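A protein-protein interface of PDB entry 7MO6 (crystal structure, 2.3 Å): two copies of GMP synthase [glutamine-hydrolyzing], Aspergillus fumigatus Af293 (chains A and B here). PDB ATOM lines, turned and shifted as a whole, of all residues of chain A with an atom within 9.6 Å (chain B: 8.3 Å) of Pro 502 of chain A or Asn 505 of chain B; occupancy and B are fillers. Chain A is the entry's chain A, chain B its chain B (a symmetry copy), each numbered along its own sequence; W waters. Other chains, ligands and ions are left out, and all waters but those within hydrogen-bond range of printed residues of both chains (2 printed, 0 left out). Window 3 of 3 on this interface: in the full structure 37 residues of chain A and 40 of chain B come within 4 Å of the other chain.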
ATOM      1  N   LEU A 455     -22.893  -1.016   1.290  1.00  0.00           N
ATOM      2  CA  LEU A 455     -24.193  -1.391   1.824  1.00  0.00           C
ATOM      3  C   LEU A 455     -24.885  -0.271   2.587  1.00  0.00           C
ATOM      4  O   LEU A 455     -25.965  -0.500   3.141  1.00  0.00           O
ATOM      5  CB  LEU A 455     -24.055  -2.611   2.745  1.00  0.00           C
ATOM      6  CG  LEU A 455     -23.208  -3.782   2.244  1.00  0.00           C
ATOM      7  CD1 LEU A 455     -23.095  -4.854   3.320  1.00  0.00           C
ATOM      8  CD2 LEU A 455     -23.782  -4.361   0.961  1.00  0.00           C
ATOM      9  N   LYS A 458     -28.277   0.630   1.078  1.00  0.00           N
ATOM     10  CA  LYS A 458     -29.200  -0.495   1.105  1.00  0.00           C
ATOM     11  C   LYS A 458     -29.712  -0.800   2.505  1.00  0.00           C
ATOM     12  O   LYS A 458     -30.452  -1.773   2.683  1.00  0.00           O
ATOM     13  CB  LYS A 458     -28.523  -1.736   0.514  1.00  0.00           C
ATOM     14  CG  LYS A 458     -27.854  -1.481  -0.830  1.00  0.00           C
ATOM     15  CD  LYS A 458     -26.927  -2.616  -1.239  1.00  0.00           C
ATOM     16  CE  LYS A 458     -27.698  -3.864  -1.637  1.00  0.00           C
ATOM     17  NZ  LYS A 458     -26.791  -4.911  -2.187  1.00  0.00           N
ATOM     18  N   ILE A 459     -29.340   0.007   3.497  1.00  0.00           N
ATOM     19  CA  ILE A 459     -29.725  -0.195   4.887  1.00  0.00           C
ATOM     20  C   ILE A 459     -30.436   1.059   5.378  1.00  0.00           C
ATOM     21  O   ILE A 459     -29.986   2.180   5.119  1.00  0.00           O
ATOM     22  CB  ILE A 459     -28.500  -0.513   5.771  1.00  0.00           C
ATOM     23  CG1 ILE A 459     -27.848  -1.825   5.330  1.00  0.00           C
ATOM     24  CG2 ILE A 459     -28.891  -0.581   7.236  1.00  0.00           C
ATOM     25  CD1 ILE A 459     -26.560  -2.142   6.065  1.00  0.00           C
ATOM     26  N   SER A 460     -31.551   0.867   6.087  1.00  0.00           N
ATOM     27  CA  SER A 460     -32.301   2.005   6.608  1.00  0.00           C
ATOM     28  C   SER A 460     -31.659   2.570   7.871  1.00  0.00           C
ATOM     29  O   SER A 460     -31.534   3.791   8.012  1.00  0.00           O
ATOM     30  CB  SER A 460     -33.750   1.599   6.879  1.00  0.00           C
ATOM     31  N   ALA A 489     -28.710  -3.580  12.288  1.00  0.00           N
ATOM     32  CA  ALA A 489     -28.844  -3.012  10.949  1.00  0.00           C
ATOM     33  C   ALA A 489     -30.094  -3.590  10.306  1.00  0.00           C
ATOM     34  O   ALA A 489     -30.231  -4.814  10.207  1.00  0.00           O
ATOM     35  CB  ALA A 489     -27.611  -3.303  10.094  1.00  0.00           C
ATOM     36  N   VAL A 490     -31.000  -2.714   9.868  1.00  0.00           N
ATOM     37  CA  VAL A 490     -32.295  -3.129   9.345  1.00  0.00           C
ATOM     38  C   VAL A 490     -32.555  -2.460   8.001  1.00  0.00           C
ATOM     39  O   VAL A 490     -32.072  -1.358   7.722  1.00  0.00           O
ATOM     40  CB  VAL A 490     -33.444  -2.809  10.330  1.00  0.00           C
ATOM     41  CG1 VAL A 490     -33.235  -3.534  11.651  1.00  0.00           C
ATOM     42  CG2 VAL A 490     -33.561  -1.308  10.550  1.00  0.00           C
ATOM     43  N   GLU A 491     -33.327  -3.148   7.165  1.00  0.00           N
ATOM     44  CA  GLU A 491     -33.841  -2.607   5.915  1.00  0.00           C
ATOM     45  C   GLU A 491     -35.326  -2.322   6.089  1.00  0.00           C
ATOM     46  O   GLU A 491     -36.078  -3.189   6.546  1.00  0.00           O
ATOM     47  CB  GLU A 491     -33.611  -3.582   4.756  1.00  0.00           C
ATOM     48  CG  GLU A 491     -33.966  -5.030   5.076  1.00  0.00           C
ATOM     49  CD  GLU A 491     -33.832  -5.951   3.877  1.00  0.00           C
ATOM     50  OE1 GLU A 491     -34.668  -6.869   3.736  1.00  0.00           O
ATOM     51  OE2 GLU A 491     -32.895  -5.755   3.075  1.00  0.00           O
ATOM     52  N   THR A 492     -35.746  -1.109   5.735  1.00  0.00           N
ATOM     53  CA  THR A 492     -37.114  -0.677   5.975  1.00  0.00           C
ATOM     54  C   THR A 492     -37.644   0.081   4.769  1.00  0.00           C
ATOM     55  O   THR A 492     -36.942   0.915   4.191  1.00  0.00           O
ATOM     56  CB  THR A 492     -37.208   0.211   7.223  1.00  0.00           C
ATOM     57  N   ALA A 498     -39.771  -3.405   8.988  1.00  0.00           N
ATOM     58  CA  ALA A 498     -38.324  -3.487   8.840  1.00  0.00           C
ATOM     59  C   ALA A 498     -37.866  -4.888   9.212  1.00  0.00           C
ATOM     60  O   ALA A 498     -38.453  -5.539  10.081  1.00  0.00           O
ATOM     61  CB  ALA A 498     -37.605  -2.445   9.707  1.00  0.00           C
ATOM     62  N   ARG A 499     -36.811  -5.345   8.544  1.00  0.00           N
ATOM     63  CA  ARG A 499     -36.214  -6.641   8.822  1.00  0.00           C
ATOM     64  C   ARG A 499     -34.716  -6.471   9.020  1.00  0.00           C
ATOM     65  O   ARG A 499     -34.097  -5.577   8.437  1.00  0.00           O
ATOM     66  CB  ARG A 499     -36.477  -7.645   7.691  1.00  0.00           C
ATOM     67  CG  ARG A 499     -36.589  -9.088   8.161  1.00  0.00           C
ATOM     68  CD  ARG A 499     -35.922 -10.058   7.196  1.00  0.00           C
ATOM     69  NE  ARG A 499     -34.506 -10.249   7.506  1.00  0.00           N
ATOM     70  CZ  ARG A 499     -33.733 -11.172   6.940  1.00  0.00           C
ATOM     71  NH1 ARG A 499     -34.236 -11.995   6.031  1.00  0.00           N
ATOM     72  NH2 ARG A 499     -32.457 -11.273   7.287  1.00  0.00           N
ATOM     73  N   ALA A 500     -34.141  -7.337   9.853  1.00  0.00           N
ATOM     74  CA  ALA A 500     -32.698  -7.337  10.047  1.00  0.00           C
ATOM     75  C   ALA A 500     -31.996  -7.565   8.715  1.00  0.00           C
ATOM     76  O   ALA A 500     -32.351  -8.476   7.962  1.00  0.00           O
ATOM     77  CB  ALA A 500     -32.297  -8.414  11.055  1.00  0.00           C
ATOM     78  N   PHE A 501     -31.010  -6.725   8.421  1.00  0.00           N
ATOM     79  CA  PHE A 501     -30.364  -6.771   7.119  1.00  0.00           C
ATOM     80  C   PHE A 501     -29.629  -8.097   6.942  1.00  0.00           C
ATOM     81  O   PHE A 501     -28.827  -8.477   7.805  1.00  0.00           O
ATOM     82  CB  PHE A 501     -29.392  -5.605   6.956  1.00  0.00           C
ATOM     83  CG  PHE A 501     -28.760  -5.536   5.597  1.00  0.00           C
ATOM     84  CD1 PHE A 501     -29.447  -4.986   4.527  1.00  0.00           C
ATOM     85  CD2 PHE A 501     -27.483  -6.026   5.386  1.00  0.00           C
ATOM     86  CE1 PHE A 501     -28.869  -4.923   3.273  1.00  0.00           C
ATOM     87  CE2 PHE A 501     -26.899  -5.967   4.136  1.00  0.00           C
ATOM     88  CZ  PHE A 501     -27.594  -5.416   3.078  1.00  0.00           C
ATOM     89  N   PRO A 502     -29.874  -8.825   5.854  1.00  0.00           N
ATOM     90  CA  PRO A 502     -29.202 -10.122   5.628  1.00  0.00           C
ATOM     91  C   PRO A 502     -27.757  -9.967   5.156  1.00  0.00           C
ATOM     92  O   PRO A 502     -27.420 -10.071   3.976  1.00  0.00           O
ATOM     93  CB  PRO A 502     -30.088 -10.775   4.564  1.00  0.00           C
ATOM     94  CG  PRO A 502     -30.645  -9.622   3.797  1.00  0.00           C
ATOM     95  CD  PRO A 502     -30.850  -8.513   4.794  1.00  0.00           C
ATOM     96  N   PHE A 503     -26.870  -9.706   6.114  1.00  0.00           N
ATOM     97  CA  PHE A 503     -25.449  -9.624   5.815  1.00  0.00           C
ATOM     98  C   PHE A 503     -24.914 -10.980   5.366  1.00  0.00           C
ATOM     99  O   PHE A 503     -25.468 -12.037   5.680  1.00  0.00           O
ATOM    100  CB  PHE A 503     -24.655  -9.168   7.041  1.00  0.00           C
ATOM    101  CG  PHE A 503     -24.865  -7.731   7.414  1.00  0.00           C
ATOM    102  CD1 PHE A 503     -24.315  -6.714   6.655  1.00  0.00           C
ATOM    103  CD2 PHE A 503     -25.586  -7.398   8.549  1.00  0.00           C
ATOM    104  CE1 PHE A 503     -24.498  -5.390   7.006  1.00  0.00           C
ATOM    105  CE2 PHE A 503     -25.771  -6.078   8.906  1.00  0.00           C
ATOM    106  CZ  PHE A 503     -25.226  -5.073   8.134  1.00  0.00           C
ATOM    107  N   ASP A 504     -23.814 -10.938   4.622  1.00  0.00           N
ATOM    108  CA  ASP A 504     -23.034 -12.145   4.398  1.00  0.00           C
ATOM    109  C   ASP A 504     -22.355 -12.536   5.704  1.00  0.00           C
ATOM    110  O   ASP A 504     -21.758 -11.693   6.379  1.00  0.00           O
ATOM    111  CB  ASP A 504     -21.996 -11.919   3.299  1.00  0.00           C
ATOM    112  CG  ASP A 504     -21.207 -13.174   2.974  1.00  0.00           C
ATOM    113  OD1 ASP A 504     -21.651 -14.278   3.355  1.00  0.00           O
ATOM    114  OD2 ASP A 504     -20.136 -13.056   2.341  1.00  0.00           O
ATOM    115  N   ASN A 505     -22.457 -13.815   6.069  1.00  0.00           N
ATOM    116  CA  ASN A 505     -21.900 -14.258   7.342  1.00  0.00           C
ATOM    117  C   ASN A 505     -20.387 -14.089   7.398  1.00  0.00           C
ATOM    118  O   ASN A 505     -19.820 -14.050   8.495  1.00  0.00           O
ATOM    119  CB  ASN A 505     -22.285 -15.714   7.608  1.00  0.00           C
ATOM    120  CG  ASN A 505     -22.956 -15.896   8.955  1.00  0.00           C
ATOM    121  OD1 ASN A 505     -22.457 -15.424   9.978  1.00  0.00           O
ATOM    122  ND2 ASN A 505     -24.101 -16.567   8.961  1.00  0.00           N
ATOM    123  N   GLU A 506     -19.723 -13.983   6.245  1.00  0.00           N
ATOM    124  CA  GLU A 506     -18.309 -13.634   6.243  1.00  0.00           C
ATOM    125  C   GLU A 506     -18.095 -12.182   6.650  1.00  0.00           C
ATOM    126  O   GLU A 506     -17.082 -11.859   7.280  1.00  0.00           O
ATOM    127  CB  GLU A 506     -17.702 -13.894   4.863  1.00  0.00           C
ATOM    128  N   PHE A 507     -19.036 -11.298   6.305  1.00  0.00           N
ATOM    129  CA  PHE A 507     -18.917  -9.898   6.699  1.00  0.00           C
ATOM    130  C   PHE A 507     -19.136  -9.725   8.197  1.00  0.00           C
ATOM    131  O   PHE A 507     -18.411  -8.968   8.852  1.00  0.00           O
ATOM    132  CB  PHE A 507     -19.909  -9.044   5.906  1.00  0.00           C
ATOM    133  CG  PHE A 507     -20.001  -7.617   6.375  1.00  0.00           C
ATOM    134  CD1 PHE A 507     -19.111  -6.661   5.910  1.00  0.00           C
ATOM    135  CD2 PHE A 507     -20.981  -7.230   7.276  1.00  0.00           C
ATOM    136  CE1 PHE A 507     -19.193  -5.348   6.338  1.00  0.00           C
ATOM    137  CE2 PHE A 507     -21.067  -5.919   7.709  1.00  0.00           C
ATOM    138  CZ  PHE A 507     -20.173  -4.977   7.239  1.00  0.00           C
ATOM    139  N   LEU A 508     -20.134 -10.414   8.755  1.00  0.00           N
ATOM    140  CA  LEU A 508     -20.408 -10.284  10.183  1.00  0.00           C
ATOM    141  C   LEU A 508     -19.306 -10.923  11.020  1.00  0.00           C
ATOM    142  O   LEU A 508     -18.969 -10.419  12.097  1.00  0.00           O
ATOM    143  CB  LEU A 508     -21.767 -10.902  10.517  1.00  0.00           C
ATOM    144  CG  LEU A 508     -23.001 -10.074  10.158  1.00  0.00           C
ATOM    145  CD1 LEU A 508     -24.261 -10.913  10.285  1.00  0.00           C
ATOM    146  CD2 LEU A 508     -23.095  -8.832  11.035  1.00  0.00           C
ATOM    147  N   TYR A 527     -25.298  -9.826  16.952  1.00  0.00           N
ATOM    148  CA  TYR A 527     -26.042  -9.179  15.881  1.00  0.00           C
ATOM    149  C   TYR A 527     -27.533  -9.375  16.111  1.00  0.00           C
ATOM    150  O   TYR A 527     -27.998 -10.508  16.271  1.00  0.00           O
ATOM    151  CB  TYR A 527     -25.638  -9.729  14.510  1.00  0.00           C
ATOM    152  CG  TYR A 527     -26.384  -9.096  13.358  1.00  0.00           C
ATOM    153  CD1 TYR A 527     -26.522  -7.716  13.270  1.00  0.00           C
ATOM    154  CD2 TYR A 527     -26.938  -9.874  12.351  1.00  0.00           C
ATOM    155  CE1 TYR A 527     -27.200  -7.131  12.217  1.00  0.00           C
ATOM    156  CE2 TYR A 527     -27.615  -9.299  11.293  1.00  0.00           C
ATOM    157  CZ  TYR A 527     -27.743  -7.927  11.232  1.00  0.00           C
ATOM    158  OH  TYR A 527     -28.418  -7.350  10.181  1.00  0.00           O
ATOM    159  N   ASP A 528     -28.275  -8.271  16.129  1.00  0.00           N
ATOM    160  CA  ASP A 528     -29.714  -8.328  16.346  1.00  0.00           C
ATOM    161  C   ASP A 528     -30.401  -8.888  15.106  1.00  0.00           C
ATOM    162  O   ASP A 528     -30.224  -8.368  13.999  1.00  0.00           O
ATOM    163  CB  ASP A 528     -30.250  -6.939  16.684  1.00  0.00           C
ATOM    164  CG  ASP A 528     -31.678  -6.969  17.201  1.00  0.00           C
ATOM    165  OD1 ASP A 528     -32.288  -8.058  17.228  1.00  0.00           O
ATOM    166  OD2 ASP A 528     -32.191  -5.898  17.591  1.00  0.00           O
ATOM    167  N   ILE A 529     -31.182  -9.950  15.292  1.00  0.00           N
ATOM    168  CA  ILE A 529     -31.919 -10.587  14.209  1.00  0.00           C
ATOM    169  C   ILE A 529     -33.428 -10.486  14.426  1.00  0.00           C
ATOM    170  O   ILE A 529     -34.191 -11.255  13.853  1.00  0.00           O
ATOM    171  CB  ILE A 529     -31.481 -12.054  14.029  1.00  0.00           C
ATOM    172  CG1 ILE A 529     -31.670 -12.833  15.332  1.00  0.00           C
ATOM    173  CG2 ILE A 529     -30.037 -12.123  13.562  1.00  0.00           C
ATOM    174  CD1 ILE A 529     -31.259 -14.286  15.241  1.00  0.00           C
ATOM    175  N   SER A 530     -33.865  -9.538  15.253  1.00  0.00           N
ATOM    176  CA  SER A 530     -35.280  -9.345  15.540  1.00  0.00           C
ATOM    177  C   SER A 530     -35.891  -8.403  14.510  1.00  0.00           C
ATOM    178  O   SER A 530     -35.333  -7.338  14.226  1.00  0.00           O
ATOM    179  CB  SER A 530     -35.474  -8.786  16.949  1.00  0.00           C
ATOM    180  OG  SER A 530     -34.878  -9.627  17.922  1.00  0.00           O
ATOM    181  N   SER A 531     -37.034  -8.797  13.959  1.00  0.00           N
ATOM    182  CA  SER A 531     -37.706  -7.994  12.952  1.00  0.00           C
ATOM    183  C   SER A 531     -38.576  -6.923  13.608  1.00  0.00           C
ATOM    184  O   SER A 531     -38.829  -6.935  14.816  1.00  0.00           O
ATOM    185  CB  SER A 531     -38.549  -8.879  12.036  1.00  0.00           C
ATOM    186  OG  SER A 531     -37.743  -9.830  11.362  1.00  0.00           O
ATOM    187  N   PRO B 502     -22.638 -20.591   9.748  1.00  0.00           N
ATOM    188  CA  PRO B 502     -23.248 -19.745   8.714  1.00  0.00           C
ATOM    189  C   PRO B 502     -24.696 -20.115   8.435  1.00  0.00           C
ATOM    190  O   PRO B 502     -25.003 -20.707   7.396  1.00  0.00           O
ATOM    191  CB  PRO B 502     -22.358 -19.997   7.492  1.00  0.00           C
ATOM    192  CG  PRO B 502     -21.833 -21.375   7.701  1.00  0.00           C
ATOM    193  CD  PRO B 502     -21.655 -21.534   9.188  1.00  0.00           C
ATOM    194  N   PHE B 503     -25.591 -19.776   9.360  1.00  0.00           N
ATOM    195  CA  PHE B 503     -27.010 -20.017   9.143  1.00  0.00           C
ATOM    196  C   PHE B 503     -27.521 -19.180   7.977  1.00  0.00           C
ATOM    197  O   PHE B 503     -27.069 -18.057   7.743  1.00  0.00           O
ATOM    198  CB  PHE B 503     -27.817 -19.678  10.397  1.00  0.00           C
ATOM    199  CG  PHE B 503     -27.752 -20.722  11.471  1.00  0.00           C
ATOM    200  CD1 PHE B 503     -28.325 -21.970  11.279  1.00  0.00           C
ATOM    201  CD2 PHE B 503     -27.145 -20.447  12.684  1.00  0.00           C
ATOM    202  CE1 PHE B 503     -28.276 -22.928  12.270  1.00  0.00           C
ATOM    203  CE2 PHE B 503     -27.094 -21.402  13.680  1.00  0.00           C
ATOM    204  CZ  PHE B 503     -27.661 -22.644  13.474  1.00  0.00           C
ATOM    205  N   ASP B 504     -28.475 -19.740   7.240  1.00  0.00           N
ATOM    206  CA  ASP B 504     -29.211 -18.938   6.275  1.00  0.00           C
ATOM    207  C   ASP B 504     -29.986 -17.853   7.010  1.00  0.00           C
ATOM    208  O   ASP B 504     -30.577 -18.094   8.066  1.00  0.00           O
ATOM    209  CB  ASP B 504     -30.158 -19.814   5.457  1.00  0.00           C
ATOM    210  CG  ASP B 504     -29.434 -20.612   4.393  1.00  0.00           C
ATOM    211  OD1 ASP B 504     -28.606 -20.019   3.669  1.00  0.00           O
ATOM    212  OD2 ASP B 504     -29.685 -21.830   4.286  1.00  0.00           O
ATOM    213  N   ASN B 505     -29.968 -16.643   6.450  1.00  0.00           N
ATOM    214  CA  ASN B 505     -30.536 -15.496   7.149  1.00  0.00           C
ATOM    215  C   ASN B 505     -32.035 -15.633   7.371  1.00  0.00           C
ATOM    216  O   ASN B 505     -32.569 -15.022   8.303  1.00  0.00           O
ATOM    217  CB  ASN B 505     -30.229 -14.217   6.374  1.00  0.00           C
ATOM    218  CG  ASN B 505     -28.760 -14.091   6.031  1.00  0.00           C
ATOM    219  OD1 ASN B 505     -27.961 -13.608   6.834  1.00  0.00           O
ATOM    220  ND2 ASN B 505     -28.393 -14.534   4.834  1.00  0.00           N
ATOM    221  N   GLU B 506     -32.727 -16.420   6.545  1.00  0.00           N
ATOM    222  CA  GLU B 506     -34.146 -16.660   6.783  1.00  0.00           C
ATOM    223  C   GLU B 506     -34.361 -17.598   7.965  1.00  0.00           C
ATOM    224  O   GLU B 506     -35.407 -17.539   8.620  1.00  0.00           O
ATOM    225  CB  GLU B 506     -34.803 -17.224   5.523  1.00  0.00           C
ATOM    226  N   PHE B 507     -33.385 -18.465   8.250  1.00  0.00           N
ATOM    227  CA  PHE B 507     -33.493 -19.355   9.402  1.00  0.00           C
ATOM    228  C   PHE B 507     -33.402 -18.576  10.709  1.00  0.00           C
ATOM    229  O   PHE B 507     -34.132 -18.868  11.664  1.00  0.00           O
ATOM    230  CB  PHE B 507     -32.402 -20.428   9.331  1.00  0.00           C
ATOM    231  CG  PHE B 507     -32.398 -21.381  10.495  1.00  0.00           C
ATOM    232  CD1 PHE B 507     -31.648 -21.112  11.629  1.00  0.00           C
ATOM    233  CD2 PHE B 507     -33.126 -22.558  10.447  1.00  0.00           C
ATOM    234  CE1 PHE B 507     -31.639 -21.987  12.698  1.00  0.00           C
ATOM    235  CE2 PHE B 507     -33.118 -23.441  11.513  1.00  0.00           C
ATOM    236  CZ  PHE B 507     -32.373 -23.154  12.640  1.00  0.00           C
ATOM    237  N   LEU B 508     -32.511 -17.585  10.771  1.00  0.00           N
ATOM    238  CA  LEU B 508     -32.338 -16.818  12.001  1.00  0.00           C
ATOM    239  C   LEU B 508     -33.539 -15.923  12.270  1.00  0.00           C
ATOM    240  O   LEU B 508     -33.968 -15.779  13.421  1.00  0.00           O
ATOM    241  CB  LEU B 508     -31.056 -15.989  11.925  1.00  0.00           C
ATOM    242  CG  LEU B 508     -29.743 -16.774  11.921  1.00  0.00           C
ATOM    243  CD1 LEU B 508     -28.567 -15.848  11.657  1.00  0.00           C
ATOM    244  CD2 LEU B 508     -29.562 -17.511  13.240  1.00  0.00           C
ATOM    245  N   SER B 509     -34.094 -15.312  11.222  1.00  0.00           N
ATOM    246  CA  SER B 509     -35.259 -14.450  11.396  1.00  0.00           C
ATOM    247  C   SER B 509     -36.476 -15.245  11.855  1.00  0.00           C
ATOM    248  O   SER B 509     -37.196 -14.816  12.763  1.00  0.00           O
ATOM    249  CB  SER B 509     -35.566 -13.712  10.094  1.00  0.00           C
ATOM    250  OG  SER B 509     -36.843 -13.101  10.150  1.00  0.00           O
ATOM    251  N   LYS B 510     -36.723 -16.405  11.237  1.00  0.00           N
ATOM    252  CA  LYS B 510     -37.871 -17.215  11.628  1.00  0.00           C
ATOM    253  C   LYS B 510     -37.719 -17.765  13.040  1.00  0.00           C
ATOM    254  O   LYS B 510     -38.714 -17.889  13.763  1.00  0.00           O
ATOM    255  CB  LYS B 510     -38.080 -18.355  10.629  1.00  0.00           C
ATOM    256  CG  LYS B 510     -38.623 -17.905   9.279  1.00  0.00           C
ATOM    257  CD  LYS B 510     -38.896 -19.092   8.366  1.00  0.00           C
ATOM    258  CE  LYS B 510     -39.516 -18.640   7.052  1.00  0.00           C
ATOM    259  NZ  LYS B 510     -39.793 -19.784   6.139  1.00  0.00           N
ATOM    260  N   CYS B 511     -36.492 -18.096  13.448  1.00  0.00           N
ATOM    261  CA  CYS B 511     -36.273 -18.560  14.814  1.00  0.00           C
ATOM    262  C   CYS B 511     -36.397 -17.414  15.810  1.00  0.00           C
ATOM    263  O   CYS B 511     -36.918 -17.599  16.915  1.00  0.00           O
ATOM    264  CB  CYS B 511     -34.901 -19.225  14.930  1.00  0.00           C
ATOM    265  SG  CYS B 511     -34.483 -19.796  16.598  1.00  0.00           S
ATOM    266  N   ALA B 512     -35.923 -16.224  15.436  1.00  0.00           N
ATOM    267  CA  ALA B 512     -36.058 -15.068  16.317  1.00  0.00           C
ATOM    268  C   ALA B 512     -37.519 -14.671  16.484  1.00  0.00           C
ATOM    269  O   ALA B 512     -37.934 -14.249  17.570  1.00  0.00           O
ATOM    270  CB  ALA B 512     -35.241 -13.896  15.777  1.00  0.00           C
ATOM    271  N   TYR B 527     -28.005 -13.097  17.765  1.00  0.00           N
ATOM    272  CA  TYR B 527     -27.170 -14.215  17.347  1.00  0.00           C
ATOM    273  C   TYR B 527     -25.711 -13.844  17.563  1.00  0.00           C
ATOM    274  O   TYR B 527     -25.242 -12.825  17.045  1.00  0.00           O
ATOM    275  CB  TYR B 527     -27.421 -14.584  15.884  1.00  0.00           C
ATOM    276  CG  TYR B 527     -26.571 -15.739  15.400  1.00  0.00           C
ATOM    277  CD1 TYR B 527     -26.544 -16.943  16.094  1.00  0.00           C
ATOM    278  CD2 TYR B 527     -25.805 -15.630  14.247  1.00  0.00           C
ATOM    279  CE1 TYR B 527     -25.774 -18.005  15.657  1.00  0.00           C
ATOM    280  CE2 TYR B 527     -25.031 -16.687  13.802  1.00  0.00           C
ATOM    281  CZ  TYR B 527     -25.019 -17.872  14.511  1.00  0.00           C
ATOM    282  OH  TYR B 527     -24.251 -18.927  14.072  1.00  0.00           O
HETATM  283  O   HOH W   1     -26.481 -13.534   2.690  1.00  0.00           O
HETATM  284  O   HOH W   2     -36.956 -11.788  12.912  1.00  0.00           O
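The backbone carbonyl oxygen of Phe 503 of chain A lies close to the side-chain amide oxygen of Asn 505 of chain B (3.2 Å).
The backbone carbonyl oxygen of Tyr 527 of chain A sits at hydrogen-bond distance from the backbone NH of Tyr 527 of chain B (3.0 Å).
Of the 24 printed residues of chain A, 7 touch a printed residue of chain B.
Printed residues of chain A that touch a printed residue of chain B: Arg 499, Pro 502, Phe 503, Asn 505, Tyr 527, Ile 529 and Ser 531.
Printed residues of chain B that touch a printed residue of chain A: Pro 502, Phe 503, Asn 505, Leu 508, Ser 509, Ala 512 and Tyr 527.
Hydrophobic or aromatic side chains of chain B that line the printed part of chain A: Leu 508, Ala 512 and Tyr 527.
Among the printed residues, no Asp or Glu carboxylate lies within 4 Å of a Lys or Arg side-chain nitrogen of the other chain.
Water W2 lies within hydrogen-bond range of OG of Ser 531 of chain A, O of Ile 529 of chain A and O of Ser 509 of chain B.
Water W1 bridges ND2 of Asn 505 of chain B (3.0 Å) and O of Phe 503 of chain A (3.5 Å).
Among the printed residues, pairs that only touch across the chains: Asn 505 of chain A with Pro 502 of chain B (3.3 Å), Ile 529 of chain A with Ala 512 of chain B (3.4 Å), Asn 505 of chain A with Phe 503 of chain B (3.5 Å), Ile 529 of chain A with Leu 508 of chain B (3.6 Å), Ser 531 of chain A with Ser 509 of chain B (3.6 Å), Arg 499 of chain A with Asn 505 of chain B (3.8 Å), Pro 502 of chain A with Asn 505 of chain B (3.9 Å) and Ile 529 of chain A with Tyr 527 of chain B (3.9 Å).
Of chain B, only Asn 505 comes within 4 Å of Pro 502 of chain A.
Of the printed residues of chain A, Asn 505 of chain B touches Arg 499, Pro 502 and Phe 503.
No residue of chain A comes within 4 Å of Glu 506 of chain B.
Printed residues of chain B within 4 Å of Arg 499 of chain A: Asn 505 (3.8 Å).
Of the printed residues of chain A, Ser 509 of chain B touches Ser 531.
Printed residues of chain A within 4 Å of Leu 508 of chain B: Ile 529 (3.6 Å).
Leu 455 of chain A touches none of the printed residues of chain B.
The nearest residue of chain B that does not touch Pro 502 of chain A is Glu 506 of chain B (6.5 Å).
The side-chain hydroxyl (OH) of Tyr 527 of chain A sits at hydrogen-bond distance from the backbone carbonyl oxygen (O) of Ala 489 of chain A, at 3.1 Å.
The backbone carbonyl oxygen (O) of Arg 499 of chain A is in hydrogen-bond range of the backbone NH (N) of Glu 491 of chain A.
The side-chain hydroxyl of Tyr 527 of chain A is in hydrogen-bond range of the backbone carbonyl oxygen of Phe 501 of chain A, 2.7 Å away.
Pro 502 of chain A touches Asn 505 of chain B, and with the chains exchanged Asn 505 of chain A touches Pro 502 of chain B.
Phe 503 of chain A touches Asn 505 of chain B, and with the chains exchanged Asn 505 of chain A touches Phe 503 of chain B.
Tyr 527 of chain A touches its own counterpart, Tyr 527 of chain B.
Positions printed for both chains: 502, 503, 504, 505, 506, 507, 508 and 527.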
